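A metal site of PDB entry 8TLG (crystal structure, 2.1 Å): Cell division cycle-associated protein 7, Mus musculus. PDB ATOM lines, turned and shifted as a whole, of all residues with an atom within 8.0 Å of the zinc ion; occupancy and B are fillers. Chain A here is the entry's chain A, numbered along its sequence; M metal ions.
The side-chain sulfur (SG) of Cys 57 sits close to the backbone NH (N) of Asn 59 (3.6 Å).
The backbone carbonyl oxygen (O) of Cys 57 is in hydrogen-bond range of a ring nitrogen (NE2) of His 10, at 2.5 Å.
The backbone carbonyl oxygen (O) of Cys 62 is in hydrogen-bond range of a ring nitrogen (ND1) of His 10 (3.2 Å).
NH1 of Arg 66 lies close to SG of Cys 96 (3.4 Å).
SG of Cys 96 sits close to ND2 of Asn 59, at 3.2 Å.
The side-chain sulfur (SG) of Cys 57 is bound to the zinc ion (2.3 Å).
SG of Cys 93 binds the zinc ion, at 2.3 Å.
The side-chain sulfur (SG) of Cys 62 is bound to the zinc ion (2.3 Å).
SG of Cys 96 binds the zinc ion.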
ATOM      1  N   HIS A  10      16.497 -11.003 -27.138  1.00  0.00           N
ATOM      2  CA  HIS A  10      16.565 -11.170 -25.699  1.00  0.00           C
ATOM      3  C   HIS A  10      16.667 -12.664 -25.381  1.00  0.00           C
ATOM      4  O   HIS A  10      15.741 -13.427 -25.644  1.00  0.00           O
ATOM      5  CB  HIS A  10      15.338 -10.555 -25.022  1.00  0.00           C
ATOM      6  CG  HIS A  10      15.160 -10.986 -23.601  1.00  0.00           C
ATOM      7  ND1 HIS A  10      14.057 -11.713 -23.179  1.00  0.00           N
ATOM      8  CD2 HIS A  10      15.937 -10.805 -22.505  1.00  0.00           C
ATOM      9  CE1 HIS A  10      14.166 -11.949 -21.881  1.00  0.00           C
ATOM     10  NE2 HIS A  10      15.294 -11.411 -21.454  1.00  0.00           N
ATOM     11  N   ASN A  56      19.848  -9.400 -16.582  1.00  0.00           N
ATOM     12  CA  ASN A  56      19.196 -10.175 -17.638  1.00  0.00           C
ATOM     13  C   ASN A  56      17.770 -10.435 -17.208  1.00  0.00           C
ATOM     14  O   ASN A  56      17.526 -11.240 -16.292  1.00  0.00           O
ATOM     15  CB  ASN A  56      19.954 -11.471 -17.901  1.00  0.00           C
ATOM     16  CG  ASN A  56      19.364 -12.264 -19.054  1.00  0.00           C
ATOM     17  OD1 ASN A  56      18.725 -13.298 -18.845  1.00  0.00           O
ATOM     18  ND2 ASN A  56      19.592 -11.797 -20.279  1.00  0.00           N
ATOM     19  N   CYS A  57      16.816  -9.754 -17.839  1.00  0.00           N
ATOM     20  CA  CYS A  57      15.411  -9.975 -17.515  1.00  0.00           C
ATOM     21  C   CYS A  57      15.006 -11.390 -17.899  1.00  0.00           C
ATOM     22  O   CYS A  57      15.258 -11.830 -19.027  1.00  0.00           O
ATOM     23  CB  CYS A  57      14.528  -8.953 -18.235  1.00  0.00           C
ATOM     24  SG  CYS A  57      12.762  -9.071 -17.830  1.00  0.00           S
ATOM     25  N   ARG A  58      14.395 -12.108 -16.963  1.00  0.00           N
ATOM     26  CA  ARG A  58      13.992 -13.488 -17.187  1.00  0.00           C
ATOM     27  C   ARG A  58      12.500 -13.615 -17.451  1.00  0.00           C
ATOM     28  O   ARG A  58      11.960 -14.718 -17.382  1.00  0.00           O
ATOM     29  CB  ARG A  58      14.426 -14.348 -16.007  1.00  0.00           C
ATOM     30  CG  ARG A  58      15.939 -14.346 -15.833  1.00  0.00           C
ATOM     31  CD  ARG A  58      16.418 -15.402 -14.868  1.00  0.00           C
ATOM     32  NE  ARG A  58      17.860 -15.600 -15.005  1.00  0.00           N
ATOM     33  CZ  ARG A  58      18.781 -14.887 -14.360  1.00  0.00           C
ATOM     34  NH1 ARG A  58      18.442 -13.927 -13.508  1.00  0.00           N
ATOM     35  NH2 ARG A  58      20.061 -15.143 -14.587  1.00  0.00           N
ATOM     36  N   ASN A  59      11.834 -12.505 -17.750  1.00  0.00           N
ATOM     37  CA  ASN A  59      10.462 -12.558 -18.232  1.00  0.00           C
ATOM     38  C   ASN A  59      10.455 -12.969 -19.696  1.00  0.00           C
ATOM     39  O   ASN A  59      11.080 -12.295 -20.516  1.00  0.00           O
ATOM     40  CB  ASN A  59       9.793 -11.198 -18.058  1.00  0.00           C
ATOM     41  CG  ASN A  59       8.354 -11.184 -18.538  1.00  0.00           C
ATOM     42  OD1 ASN A  59       7.732 -12.230 -18.700  1.00  0.00           O
ATOM     43  ND2 ASN A  59       7.828  -9.987 -18.771  1.00  0.00           N
ATOM     44  N   PRO A  60       9.793 -14.075 -20.062  1.00  0.00           N
ATOM     45  CA  PRO A  60       9.814 -14.507 -21.468  1.00  0.00           C
ATOM     46  C   PRO A  60       9.242 -13.488 -22.438  1.00  0.00           C
ATOM     47  O   PRO A  60       9.639 -13.482 -23.609  1.00  0.00           O
ATOM     48  CB  PRO A  60       8.992 -15.801 -21.445  1.00  0.00           C
ATOM     49  CG  PRO A  60       9.093 -16.289 -20.032  1.00  0.00           C
ATOM     50  CD  PRO A  60       9.126 -15.053 -19.185  1.00  0.00           C
ATOM     51  N   ASP A  61       8.330 -12.640 -21.998  1.00  0.00           N
ATOM     52  CA  ASP A  61       7.728 -11.643 -22.882  1.00  0.00           C
ATOM     53  C   ASP A  61       8.551 -10.373 -22.987  1.00  0.00           C
ATOM     54  O   ASP A  61       8.161  -9.458 -23.718  1.00  0.00           O
ATOM     55  CB  ASP A  61       6.302 -11.299 -22.404  1.00  0.00           C
ATOM     56  CG  ASP A  61       5.463 -10.679 -23.509  1.00  0.00           C
ATOM     57  OD1 ASP A  61       5.868 -10.748 -24.680  1.00  0.00           O
ATOM     58  OD2 ASP A  61       4.387 -10.118 -23.188  1.00  0.00           O
ATOM     59  N   CYS A  62       9.676 -10.283 -22.278  1.00  0.00           N
ATOM     60  CA  CYS A  62      10.571  -9.161 -22.449  1.00  0.00           C
ATOM     61  C   CYS A  62      11.293  -9.254 -23.792  1.00  0.00           C
ATOM     62  O   CYS A  62      11.395 -10.321 -24.397  1.00  0.00           O
ATOM     63  CB  CYS A  62      11.582  -9.104 -21.299  1.00  0.00           C
ATOM     64  SG  CYS A  62      12.353  -7.490 -21.046  1.00  0.00           S
ATOM     65  N   TRP A  63      11.775  -8.110 -24.278  1.00  0.00           N
ATOM     66  CA  TRP A  63      12.439  -8.062 -25.567  1.00  0.00           C
ATOM     67  C   TRP A  63      13.470  -6.958 -25.561  1.00  0.00           C
ATOM     68  O   TRP A  63      13.382  -5.996 -24.792  1.00  0.00           O
ATOM     69  CB  TRP A  63      11.432  -7.841 -26.707  1.00  0.00           C
ATOM     70  CG  TRP A  63      10.900  -6.441 -26.749  1.00  0.00           C
ATOM     71  CD1 TRP A  63      11.352  -5.420 -27.539  1.00  0.00           C
ATOM     72  CD2 TRP A  63       9.826  -5.901 -25.974  1.00  0.00           C
ATOM     73  NE1 TRP A  63      10.619  -4.281 -27.297  1.00  0.00           N
ATOM     74  CE2 TRP A  63       9.680  -4.549 -26.333  1.00  0.00           C
ATOM     75  CE3 TRP A  63       8.977  -6.436 -24.999  1.00  0.00           C
ATOM     76  CZ2 TRP A  63       8.712  -3.729 -25.769  1.00  0.00           C
ATOM     77  CZ3 TRP A  63       8.022  -5.619 -24.434  1.00  0.00           C
ATOM     78  CH2 TRP A  63       7.892  -4.276 -24.819  1.00  0.00           C
ATOM     79  N   GLY A  64      14.462  -7.098 -26.436  1.00  0.00           N
ATOM     80  CA  GLY A  64      15.446  -6.048 -26.614  1.00  0.00           C
ATOM     81  C   GLY A  64      16.305  -5.833 -25.380  1.00  0.00           C
ATOM     82  O   GLY A  64      16.575  -6.751 -24.591  1.00  0.00           O
ATOM     83  N   ILE A  65      16.740  -4.577 -25.201  1.00  0.00           N
ATOM     84  CA  ILE A  65      17.693  -4.221 -24.152  1.00  0.00           C
ATOM     85  C   ILE A  65      17.002  -3.554 -22.965  1.00  0.00           C
ATOM     86  O   ILE A  65      17.692  -3.107 -22.035  1.00  0.00           O
ATOM     87  CB  ILE A  65      18.806  -3.320 -24.697  1.00  0.00           C
ATOM     88  CG1 ILE A  65      18.218  -1.971 -25.108  1.00  0.00           C
ATOM     89  CG2 ILE A  65      19.491  -3.984 -25.877  1.00  0.00           C
ATOM     90  CD1 ILE A  65      19.226  -0.859 -25.163  1.00  0.00           C
ATOM     91  N   ARG A  66      15.672  -3.468 -22.963  1.00  0.00           N
ATOM     92  CA  ARG A  66      14.972  -2.769 -21.896  1.00  0.00           C
ATOM     93  C   ARG A  66      15.216  -3.404 -20.533  1.00  0.00           C
ATOM     94  O   ARG A  66      15.032  -2.731 -19.508  1.00  0.00           O
ATOM     95  CB  ARG A  66      13.468  -2.724 -22.194  1.00  0.00           C
ATOM     96  CG  ARG A  66      12.758  -4.050 -21.983  1.00  0.00           C
ATOM     97  CD  ARG A  66      11.521  -4.186 -22.858  1.00  0.00           C
ATOM     98  NE  ARG A  66      10.424  -3.326 -22.425  1.00  0.00           N
ATOM     99  CZ  ARG A  66       9.460  -3.709 -21.590  1.00  0.00           C
ATOM    100  NH1 ARG A  66       9.446  -4.918 -21.055  1.00  0.00           N
ATOM    101  NH2 ARG A  66       8.489  -2.851 -21.302  1.00  0.00           N
ATOM    102  N   GLY A  67      15.606  -4.672 -20.495  1.00  0.00           N
ATOM    103  CA  GLY A  67      15.893  -5.363 -19.263  1.00  0.00           C
ATOM    104  C   GLY A  67      17.322  -5.310 -18.781  1.00  0.00           C
ATOM    105  O   GLY A  67      17.640  -5.940 -17.764  1.00  0.00           O
ATOM    106  N   GLN A  68      18.205  -4.584 -19.465  1.00  0.00           N
ATOM    107  CA  GLN A  68      19.619  -4.549 -19.132  1.00  0.00           C
ATOM    108  C   GLN A  68      19.914  -3.308 -18.311  1.00  0.00           C
ATOM    109  O   GLN A  68      19.738  -2.185 -18.796  1.00  0.00           O
ATOM    110  CB  GLN A  68      20.478  -4.575 -20.403  1.00  0.00           C
ATOM    111  CG  GLN A  68      20.223  -5.780 -21.292  1.00  0.00           C
ATOM    112  CD  GLN A  68      21.012  -5.712 -22.576  1.00  0.00           C
ATOM    113  OE1 GLN A  68      21.727  -4.750 -22.837  1.00  0.00           O
ATOM    114  NE2 GLN A  68      20.881  -6.751 -23.393  1.00  0.00           N
ATOM    115  N   PHE A  69      20.387  -3.506 -17.084  1.00  0.00           N
ATOM    116  CA  PHE A  69      20.699  -2.421 -16.167  1.00  0.00           C
ATOM    117  C   PHE A  69      22.085  -2.619 -15.592  1.00  0.00           C
ATOM    118  O   PHE A  69      22.457  -3.737 -15.222  1.00  0.00           O
ATOM    119  CB  PHE A  69      19.658  -2.335 -15.034  1.00  0.00           C
ATOM    120  CG  PHE A  69      18.319  -1.814 -15.480  1.00  0.00           C
ATOM    121  CD1 PHE A  69      17.434  -2.632 -16.175  1.00  0.00           C
ATOM    122  CD2 PHE A  69      17.944  -0.507 -15.220  1.00  0.00           C
ATOM    123  CE1 PHE A  69      16.213  -2.157 -16.590  1.00  0.00           C
ATOM    124  CE2 PHE A  69      16.716  -0.028 -15.629  1.00  0.00           C
ATOM    125  CZ  PHE A  69      15.852  -0.848 -16.316  1.00  0.00           C
ATOM    126  N   TRP A  91      13.641 -12.883 -11.637  1.00  0.00           N
ATOM    127  CA  TRP A  91      13.828 -11.442 -11.684  1.00  0.00           C
ATOM    128  C   TRP A  91      13.274 -10.868 -12.984  1.00  0.00           C
ATOM    129  O   TRP A  91      13.571 -11.366 -14.064  1.00  0.00           O
ATOM    130  CB  TRP A  91      15.311 -11.081 -11.532  1.00  0.00           C
ATOM    131  CG  TRP A  91      15.558  -9.610 -11.432  1.00  0.00           C
ATOM    132  CD1 TRP A  91      15.527  -8.842 -10.299  1.00  0.00           C
ATOM    133  CD2 TRP A  91      15.878  -8.719 -12.511  1.00  0.00           C
ATOM    134  NE1 TRP A  91      15.802  -7.534 -10.608  1.00  0.00           N
ATOM    135  CE2 TRP A  91      16.027  -7.429 -11.957  1.00  0.00           C
ATOM    136  CE3 TRP A  91      16.059  -8.877 -13.889  1.00  0.00           C
ATOM    137  CZ2 TRP A  91      16.343  -6.312 -12.726  1.00  0.00           C
ATOM    138  CZ3 TRP A  91      16.372  -7.779 -14.653  1.00  0.00           C
ATOM    139  CH2 TRP A  91      16.508  -6.511 -14.071  1.00  0.00           C
ATOM    140  N   HIS A  92      12.470  -9.812 -12.859  1.00  0.00           N
ATOM    141  CA  HIS A  92      11.931  -9.089 -13.994  1.00  0.00           C
ATOM    142  C   HIS A  92      12.427  -7.649 -13.947  1.00  0.00           C
ATOM    143  O   HIS A  92      12.563  -7.065 -12.868  1.00  0.00           O
ATOM    144  CB  HIS A  92      10.395  -9.112 -13.994  1.00  0.00           C
ATOM    145  CG  HIS A  92       9.807 -10.464 -14.281  1.00  0.00           C
ATOM    146  ND1 HIS A  92      10.582 -11.590 -14.453  1.00  0.00           N
ATOM    147  CD2 HIS A  92       8.526 -10.862 -14.427  1.00  0.00           C
ATOM    148  CE1 HIS A  92       9.794 -12.627 -14.694  1.00  0.00           C
ATOM    149  NE2 HIS A  92       8.548 -12.216 -14.680  1.00  0.00           N
ATOM    150  N   CYS A  93      12.696  -7.092 -15.123  1.00  0.00           N
ATOM    151  CA  CYS A  93      13.235  -5.745 -15.188  1.00  0.00           C
ATOM    152  C   CYS A  93      12.194  -4.723 -14.742  1.00  0.00           C
ATOM    153  O   CYS A  93      10.993  -4.991 -14.784  1.00  0.00           O
ATOM    154  CB  CYS A  93      13.702  -5.431 -16.608  1.00  0.00           C
ATOM    155  SG  CYS A  93      12.381  -5.266 -17.819  1.00  0.00           S
ATOM    156  N   PRO A  94      12.639  -3.550 -14.289  1.00  0.00           N
ATOM    157  CA  PRO A  94      11.698  -2.506 -13.883  1.00  0.00           C
ATOM    158  C   PRO A  94      10.724  -2.123 -14.989  1.00  0.00           C
ATOM    159  O   PRO A  94       9.546  -1.881 -14.705  1.00  0.00           O
ATOM    160  CB  PRO A  94      12.623  -1.331 -13.510  1.00  0.00           C
ATOM    161  CG  PRO A  94      13.881  -1.993 -13.055  1.00  0.00           C
ATOM    162  CD  PRO A  94      14.029  -3.226 -13.921  1.00  0.00           C
ATOM    163  N   PRO A  95      11.153  -2.058 -16.264  1.00  0.00           N
ATOM    164  CA  PRO A  95      10.148  -1.837 -17.324  1.00  0.00           C
ATOM    165  C   PRO A  95       9.067  -2.906 -17.356  1.00  0.00           C
ATOM    166  O   PRO A  95       7.897  -2.567 -17.584  1.00  0.00           O
ATOM    167  CB  PRO A  95      10.996  -1.841 -18.601  1.00  0.00           C
ATOM    168  CG  PRO A  95      12.297  -1.299 -18.158  1.00  0.00           C
ATOM    169  CD  PRO A  95      12.518  -1.901 -16.806  1.00  0.00           C
ATOM    170  N   CYS A  96       9.425  -4.173 -17.149  1.00  0.00           N
ATOM    171  CA  CYS A  96       8.406  -5.219 -17.090  1.00  0.00           C
ATOM    172  C   CYS A  96       7.470  -5.012 -15.902  1.00  0.00           C
ATOM    173  O   CYS A  96       6.253  -5.192 -16.020  1.00  0.00           O
ATOM    174  CB  CYS A  96       9.055  -6.602 -17.022  1.00  0.00           C
ATOM    175  SG  CYS A  96       9.536  -7.288 -18.642  1.00  0.00           S
ATOM    176  N   ARG A  97       8.027  -4.627 -14.759  1.00  0.00           N
ATOM    177  CA  ARG A  97       7.233  -4.380 -13.557  1.00  0.00           C
ATOM    178  C   ARG A  97       6.470  -3.065 -13.608  1.00  0.00           C
ATOM    179  O   ARG A  97       5.670  -2.805 -12.704  1.00  0.00           O
ATOM    180  CB  ARG A  97       8.128  -4.413 -12.317  1.00  0.00           C
ATOM    181  CG  ARG A  97       8.642  -5.794 -11.958  1.00  0.00           C
ATOM    182  CD  ARG A  97       9.554  -5.742 -10.742  1.00  0.00           C
ATOM    183  NE  ARG A  97      10.946  -5.535 -11.121  1.00  0.00           N
ATOM    184  CZ  ARG A  97      11.916  -5.245 -10.259  1.00  0.00           C
ATOM    185  NH1 ARG A  97      11.668  -5.088  -8.970  1.00  0.00           N
ATOM    186  NH2 ARG A  97      13.155  -5.112 -10.708  1.00  0.00           N
HETATM  187 ZN    ZN M   1      11.856  -7.239 -18.804  1.00  0.00          ZN
